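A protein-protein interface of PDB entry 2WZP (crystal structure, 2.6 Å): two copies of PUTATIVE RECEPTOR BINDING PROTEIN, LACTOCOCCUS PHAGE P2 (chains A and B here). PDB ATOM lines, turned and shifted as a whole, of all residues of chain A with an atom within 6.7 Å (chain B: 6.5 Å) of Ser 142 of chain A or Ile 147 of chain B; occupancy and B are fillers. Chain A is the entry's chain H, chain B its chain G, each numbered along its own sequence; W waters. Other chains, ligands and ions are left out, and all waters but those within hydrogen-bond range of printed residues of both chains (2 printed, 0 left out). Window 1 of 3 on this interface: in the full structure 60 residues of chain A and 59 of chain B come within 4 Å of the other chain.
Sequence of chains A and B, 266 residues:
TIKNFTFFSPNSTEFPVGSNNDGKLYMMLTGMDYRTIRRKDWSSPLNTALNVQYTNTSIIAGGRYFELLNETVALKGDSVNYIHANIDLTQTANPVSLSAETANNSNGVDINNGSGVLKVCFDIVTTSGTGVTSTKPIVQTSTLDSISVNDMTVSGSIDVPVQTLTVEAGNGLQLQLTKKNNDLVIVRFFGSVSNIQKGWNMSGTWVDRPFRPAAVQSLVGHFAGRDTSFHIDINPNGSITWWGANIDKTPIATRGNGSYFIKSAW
Water W2 bridges the backbone carbonyl oxygen (O) of Leu 144 of chain A (2.7 Å) and the side-chain hydroxyl (OG) of Ser 148 of chain B (2.8 Å). Water W1 lies within hydrogen-bond range of the backbone carbonyl oxygen (O) of Gln 140 of chain A (2.8 Å), the side-chain hydroxyl (OG) of Ser 142 of chain A (2.8 Å) and the backbone NH (N) of Asp 145 of chain B (3.0 Å).
Positions printed for both chains: 144 and 147.
Ser 142 of chain A touches just these residues of chain B: Leu 144, Ser 146, Ile 147 and Ser 148. Of chain A, only Ser 142 comes within 4 Å of Ile 147 of chain B. Printed residues of chain B within 4 Å of Leu 144 of chain A: Ser 148 (2.7 Å) and Val 149 (3.6 Å). Of the printed residues of chain A, Asp 145 of chain B touches Gln 140. Thr 30 of chain A touches none of the printed residues of chain B. Thr 36 of chain A touches none of the printed residues of chain B. The nearest printed residue of chain A that does not touch Val 149 of chain B is Ser 142 of chain A (5.5 Å).
Printed residues of chain B that touch a printed residue of chain A: Leu 144, Asp 145, Ser 146, Ile 147, Ser 148 and Val 149. Hydrophobic or aromatic side chains of chain B that line the printed part of chain A: Leu 144 and Val 149.
O of Ser 146 of chain B touches CA of Thr 141 of chain A, at 3.4 Å. Ser 142 of chain A touches Leu 144 of chain B. O of Ser 142 of chain A touches CA of Ile 147 of chain B (3.4 Å). O of Ser 148 of chain B touches C of Thr 143 of chain A, at 3.7 Å. Leu 144 of chain A touches Val 149 of chain B. Val 149 of chain B touches Ile 147 of chain A.
OD2 of Asp 145 of chain B lies within hydrogen-bond range of N of Gln 140 of chain A, at 3.0 Å. The backbone NH (N) of Ser 146 of chain B is in hydrogen-bond range of the backbone carbonyl oxygen (O) of Gln 140 of chain A. N of Ser 142 of chain A lies within hydrogen-bond range of O of Ser 146 of chain B (2.8 Å). O of Ser 142 of chain A is in hydrogen-bond range of N of Ser 148 of chain B (2.9 Å). N of Leu 144 of chain A is in hydrogen-bond range of O of Ser 148 of chain B.
The backbone carbonyl oxygen (O) of Gly 31 of chain A is in hydrogen-bond range of the backbone NH (N) of Thr 143 of chain A (2.8 Å). OG1 of Thr 36 of chain A is in hydrogen-bond range of N of Thr 141 of chain A. The backbone carbonyl oxygen (O) of Thr 141 of chain A is in hydrogen-bond range of the guanidinium group (NH2) of Arg 38 of chain A (2.9 Å).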
ATOM      1  N   THR A  30      -6.998 -24.537  22.333  1.00  0.00           N
ATOM      2  CA  THR A  30      -7.175 -23.088  22.407  1.00  0.00           C
ATOM      3  C   THR A  30      -8.129 -22.495  21.362  1.00  0.00           C
ATOM      4  O   THR A  30      -8.575 -21.348  21.506  1.00  0.00           O
ATOM      5  CB  THR A  30      -5.823 -22.372  22.463  1.00  0.00           C
ATOM      6  OG1 THR A  30      -6.020 -21.060  22.977  1.00  0.00           O
ATOM      7  CG2 THR A  30      -5.133 -22.301  21.126  1.00  0.00           C
ATOM      8  N   GLY A  31      -8.410 -23.265  20.319  1.00  0.00           N
ATOM      9  CA  GLY A  31      -9.255 -22.803  19.229  1.00  0.00           C
ATOM     10  C   GLY A  31      -8.552 -21.772  18.369  1.00  0.00           C
ATOM     11  O   GLY A  31      -9.081 -20.679  18.152  1.00  0.00           O
ATOM     12  N   MET A  32      -7.330 -22.094  17.896  1.00  0.00           N
ATOM     13  CA  MET A  32      -6.584 -21.206  17.020  1.00  0.00           C
ATOM     14  C   MET A  32      -6.365 -21.846  15.651  1.00  0.00           C
ATOM     15  O   MET A  32      -6.283 -23.077  15.527  1.00  0.00           O
ATOM     16  CB  MET A  32      -5.256 -20.762  17.665  1.00  0.00           C
ATOM     17  CG  MET A  32      -4.157 -21.813  17.599  1.00  0.00           C
ATOM     18  SD  MET A  32      -2.609 -21.366  18.430  1.00  0.00           S
ATOM     19  CE  MET A  32      -2.073 -20.039  17.423  1.00  0.00           C
ATOM     20  N   THR A  36      -3.485 -16.797  13.335  1.00  0.00           N
ATOM     21  CA  THR A  36      -3.449 -16.089  14.601  1.00  0.00           C
ATOM     22  C   THR A  36      -2.343 -16.631  15.486  1.00  0.00           C
ATOM     23  O   THR A  36      -1.609 -17.546  15.095  1.00  0.00           O
ATOM     24  CB  THR A  36      -4.837 -16.098  15.257  1.00  0.00           C
ATOM     25  OG1 THR A  36      -4.881 -15.062  16.222  1.00  0.00           O
ATOM     26  CG2 THR A  36      -5.203 -17.455  15.891  1.00  0.00           C
ATOM     27  N   ARG A  38      -1.029 -16.907  19.987  1.00  0.00           N
ATOM     28  CA  ARG A  38      -1.201 -16.717  21.414  1.00  0.00           C
ATOM     29  C   ARG A  38       0.107 -16.004  21.746  1.00  0.00           C
ATOM     30  O   ARG A  38       1.155 -16.378  21.226  1.00  0.00           O
ATOM     31  CB  ARG A  38      -1.414 -17.998  22.219  1.00  0.00           C
ATOM     32  CG  ARG A  38      -2.738 -18.698  21.951  1.00  0.00           C
ATOM     33  CD  ARG A  38      -3.998 -17.853  22.183  1.00  0.00           C
ATOM     34  NE  ARG A  38      -5.213 -18.559  21.754  1.00  0.00           N
ATOM     35  CZ  ARG A  38      -5.869 -18.318  20.627  1.00  0.00           C
ATOM     36  NH1 ARG A  38      -5.469 -17.349  19.814  1.00  0.00           N
ATOM     37  NH2 ARG A  38      -6.933 -19.042  20.305  1.00  0.00           N
ATOM     38  N   GLN A 140      -5.667 -11.827  19.023  1.00  0.00           N
ATOM     39  CA  GLN A 140      -5.544 -13.248  19.243  1.00  0.00           C
ATOM     40  C   GLN A 140      -6.974 -13.787  19.067  1.00  0.00           C
ATOM     41  O   GLN A 140      -7.853 -13.486  19.860  1.00  0.00           O
ATOM     42  CB  GLN A 140      -4.953 -13.531  20.645  1.00  0.00           C
ATOM     43  CG  GLN A 140      -3.488 -13.084  20.790  1.00  0.00           C
ATOM     44  CD  GLN A 140      -2.925 -13.207  22.160  1.00  0.00           C
ATOM     45  OE1 GLN A 140      -3.039 -14.238  22.820  1.00  0.00           O
ATOM     46  NE2 GLN A 140      -2.277 -12.152  22.609  1.00  0.00           N
ATOM     47  N   THR A 141      -7.223 -14.520  17.992  1.00  0.00           N
ATOM     48  CA  THR A 141      -8.555 -15.083  17.704  1.00  0.00           C
ATOM     49  C   THR A 141      -8.795 -16.478  18.318  1.00  0.00           C
ATOM     50  O   THR A 141      -7.966 -17.372  18.199  1.00  0.00           O
ATOM     51  CB  THR A 141      -8.807 -15.086  16.194  1.00  0.00           C
ATOM     52  OG1 THR A 141      -8.613 -13.760  15.703  1.00  0.00           O
ATOM     53  CG2 THR A 141     -10.207 -15.577  15.829  1.00  0.00           C
ATOM     54  N   SER A 142      -9.947 -16.646  18.957  1.00  0.00           N
ATOM     55  CA  SER A 142     -10.430 -17.899  19.515  1.00  0.00           C
ATOM     56  C   SER A 142     -11.645 -18.312  18.652  1.00  0.00           C
ATOM     57  O   SER A 142     -12.667 -17.618  18.610  1.00  0.00           O
ATOM     58  CB  SER A 142     -10.840 -17.727  20.973  1.00  0.00           C
ATOM     59  OG  SER A 142      -9.717 -17.476  21.802  1.00  0.00           O
ATOM     60  N   THR A 143     -11.501 -19.396  17.897  1.00  0.00           N
ATOM     61  CA  THR A 143     -12.587 -19.919  17.065  1.00  0.00           C
ATOM     62  C   THR A 143     -13.276 -21.044  17.842  1.00  0.00           C
ATOM     63  O   THR A 143     -12.686 -22.108  18.040  1.00  0.00           O
ATOM     64  CB  THR A 143     -12.055 -20.336  15.707  1.00  0.00           C
ATOM     65  OG1 THR A 143     -11.429 -19.205  15.097  1.00  0.00           O
ATOM     66  CG2 THR A 143     -13.124 -20.884  14.816  1.00  0.00           C
ATOM     67  N   LEU A 144     -14.498 -20.785  18.336  1.00  0.00           N
ATOM     68  CA  LEU A 144     -15.242 -21.743  19.149  1.00  0.00           C
ATOM     69  C   LEU A 144     -16.568 -22.203  18.535  1.00  0.00           C
ATOM     70  O   LEU A 144     -17.019 -21.609  17.563  1.00  0.00           O
ATOM     71  CB  LEU A 144     -15.382 -21.237  20.595  1.00  0.00           C
ATOM     72  CG  LEU A 144     -14.061 -20.771  21.251  1.00  0.00           C
ATOM     73  CD1 LEU A 144     -14.305 -20.143  22.580  1.00  0.00           C
ATOM     74  CD2 LEU A 144     -13.079 -21.911  21.414  1.00  0.00           C
ATOM     75  N   ILE A 147     -20.637 -22.512  23.344  1.00  0.00           N
ATOM     76  CA  ILE A 147     -20.126 -22.065  24.650  1.00  0.00           C
ATOM     77  C   ILE A 147     -21.228 -22.074  25.703  1.00  0.00           C
ATOM     78  O   ILE A 147     -22.334 -21.594  25.473  1.00  0.00           O
ATOM     79  CB  ILE A 147     -19.461 -20.651  24.569  1.00  0.00           C
ATOM     80  CG1 ILE A 147     -18.176 -20.657  23.750  1.00  0.00           C
ATOM     81  CG2 ILE A 147     -19.199 -20.043  25.945  1.00  0.00           C
ATOM     82  CD1 ILE A 147     -17.672 -19.217  23.461  1.00  0.00           C
ATOM     83  N   MET A 152     -20.036 -12.963  31.458  1.00  0.00           N
ATOM     84  CA  MET A 152     -19.153 -12.445  30.419  1.00  0.00           C
ATOM     85  C   MET A 152     -19.041 -10.933  30.451  1.00  0.00           C
ATOM     86  O   MET A 152     -20.028 -10.260  30.696  1.00  0.00           O
ATOM     87  CB  MET A 152     -19.612 -12.902  29.028  1.00  0.00           C
ATOM     88  CG  MET A 152     -18.686 -12.435  27.923  1.00  0.00           C
ATOM     89  SD  MET A 152     -19.179 -13.021  26.296  1.00  0.00           S
ATOM     90  CE  MET A 152     -18.741 -14.684  26.456  1.00  0.00           C
ATOM     91  N   LEU B 144      -9.934 -13.766  26.943  1.00  0.00           N
ATOM     92  CA  LEU B 144      -9.847 -13.939  25.497  1.00  0.00           C
ATOM     93  C   LEU B 144      -9.893 -12.612  24.746  1.00  0.00           C
ATOM     94  O   LEU B 144     -10.242 -11.583  25.336  1.00  0.00           O
ATOM     95  CB  LEU B 144     -10.897 -14.943  25.003  1.00  0.00           C
ATOM     96  CG  LEU B 144     -10.980 -16.251  25.836  1.00  0.00           C
ATOM     97  CD1 LEU B 144     -12.187 -17.053  25.474  1.00  0.00           C
ATOM     98  CD2 LEU B 144      -9.700 -17.092  25.714  1.00  0.00           C
ATOM     99  N   ASP B 145      -9.448 -12.604  23.483  1.00  0.00           N
ATOM    100  CA  ASP B 145      -9.403 -11.370  22.721  1.00  0.00           C
ATOM    101  C   ASP B 145     -10.600 -11.261  21.784  1.00  0.00           C
ATOM    102  O   ASP B 145     -11.572 -10.593  22.126  1.00  0.00           O
ATOM    103  CB  ASP B 145      -8.060 -11.255  21.998  1.00  0.00           C
ATOM    104  CG  ASP B 145      -7.699  -9.901  21.426  1.00  0.00           C
ATOM    105  OD1 ASP B 145      -8.576  -8.998  21.397  1.00  0.00           O
ATOM    106  OD2 ASP B 145      -6.536  -9.724  21.051  1.00  0.00           O
ATOM    107  N   SER B 146     -10.546 -11.899  20.613  1.00  0.00           N
ATOM    108  CA  SER B 146     -11.651 -11.895  19.669  1.00  0.00           C
ATOM    109  C   SER B 146     -12.192 -13.318  19.535  1.00  0.00           C
ATOM    110  O   SER B 146     -11.413 -14.230  19.298  1.00  0.00           O
ATOM    111  CB  SER B 146     -11.208 -11.354  18.322  1.00  0.00           C
ATOM    112  OG  SER B 146     -12.290 -11.377  17.401  1.00  0.00           O
ATOM    113  N   ILE B 147     -13.512 -13.516  19.737  1.00  0.00           N
ATOM    114  CA  ILE B 147     -14.168 -14.830  19.718  1.00  0.00           C
ATOM    115  C   ILE B 147     -15.100 -14.952  18.546  1.00  0.00           C
ATOM    116  O   ILE B 147     -15.881 -14.063  18.279  1.00  0.00           O
ATOM    117  CB  ILE B 147     -14.934 -15.099  21.063  1.00  0.00           C
ATOM    118  CG1 ILE B 147     -13.990 -15.345  22.214  1.00  0.00           C
ATOM    119  CG2 ILE B 147     -15.952 -16.249  20.975  1.00  0.00           C
ATOM    120  CD1 ILE B 147     -14.759 -15.354  23.577  1.00  0.00           C
ATOM    121  N   SER B 148     -15.070 -16.093  17.904  1.00  0.00           N
ATOM    122  CA  SER B 148     -15.985 -16.493  16.852  1.00  0.00           C
ATOM    123  C   SER B 148     -16.736 -17.696  17.469  1.00  0.00           C
ATOM    124  O   SER B 148     -16.099 -18.685  17.842  1.00  0.00           O
ATOM    125  CB  SER B 148     -15.204 -16.917  15.614  1.00  0.00           C
ATOM    126  OG  SER B 148     -15.927 -17.880  14.866  1.00  0.00           O
ATOM    127  N   VAL B 149     -18.059 -17.579  17.643  1.00  0.00           N
ATOM    128  CA  VAL B 149     -18.868 -18.635  18.248  1.00  0.00           C
ATOM    129  C   VAL B 149     -20.129 -18.946  17.434  1.00  0.00           C
ATOM    130  O   VAL B 149     -20.616 -18.081  16.704  1.00  0.00           O
ATOM    131  CB  VAL B 149     -19.150 -18.324  19.742  1.00  0.00           C
ATOM    132  CG1 VAL B 149     -20.109 -17.167  19.909  1.00  0.00           C
ATOM    133  CG2 VAL B 149     -19.673 -19.539  20.477  1.00  0.00           C
HETATM  134  O   HOH W   1      -8.369 -15.019  22.133  1.00  0.00           O
HETATM  135  O   HOH W   2     -16.733 -20.521  15.132  1.00  0.00           O
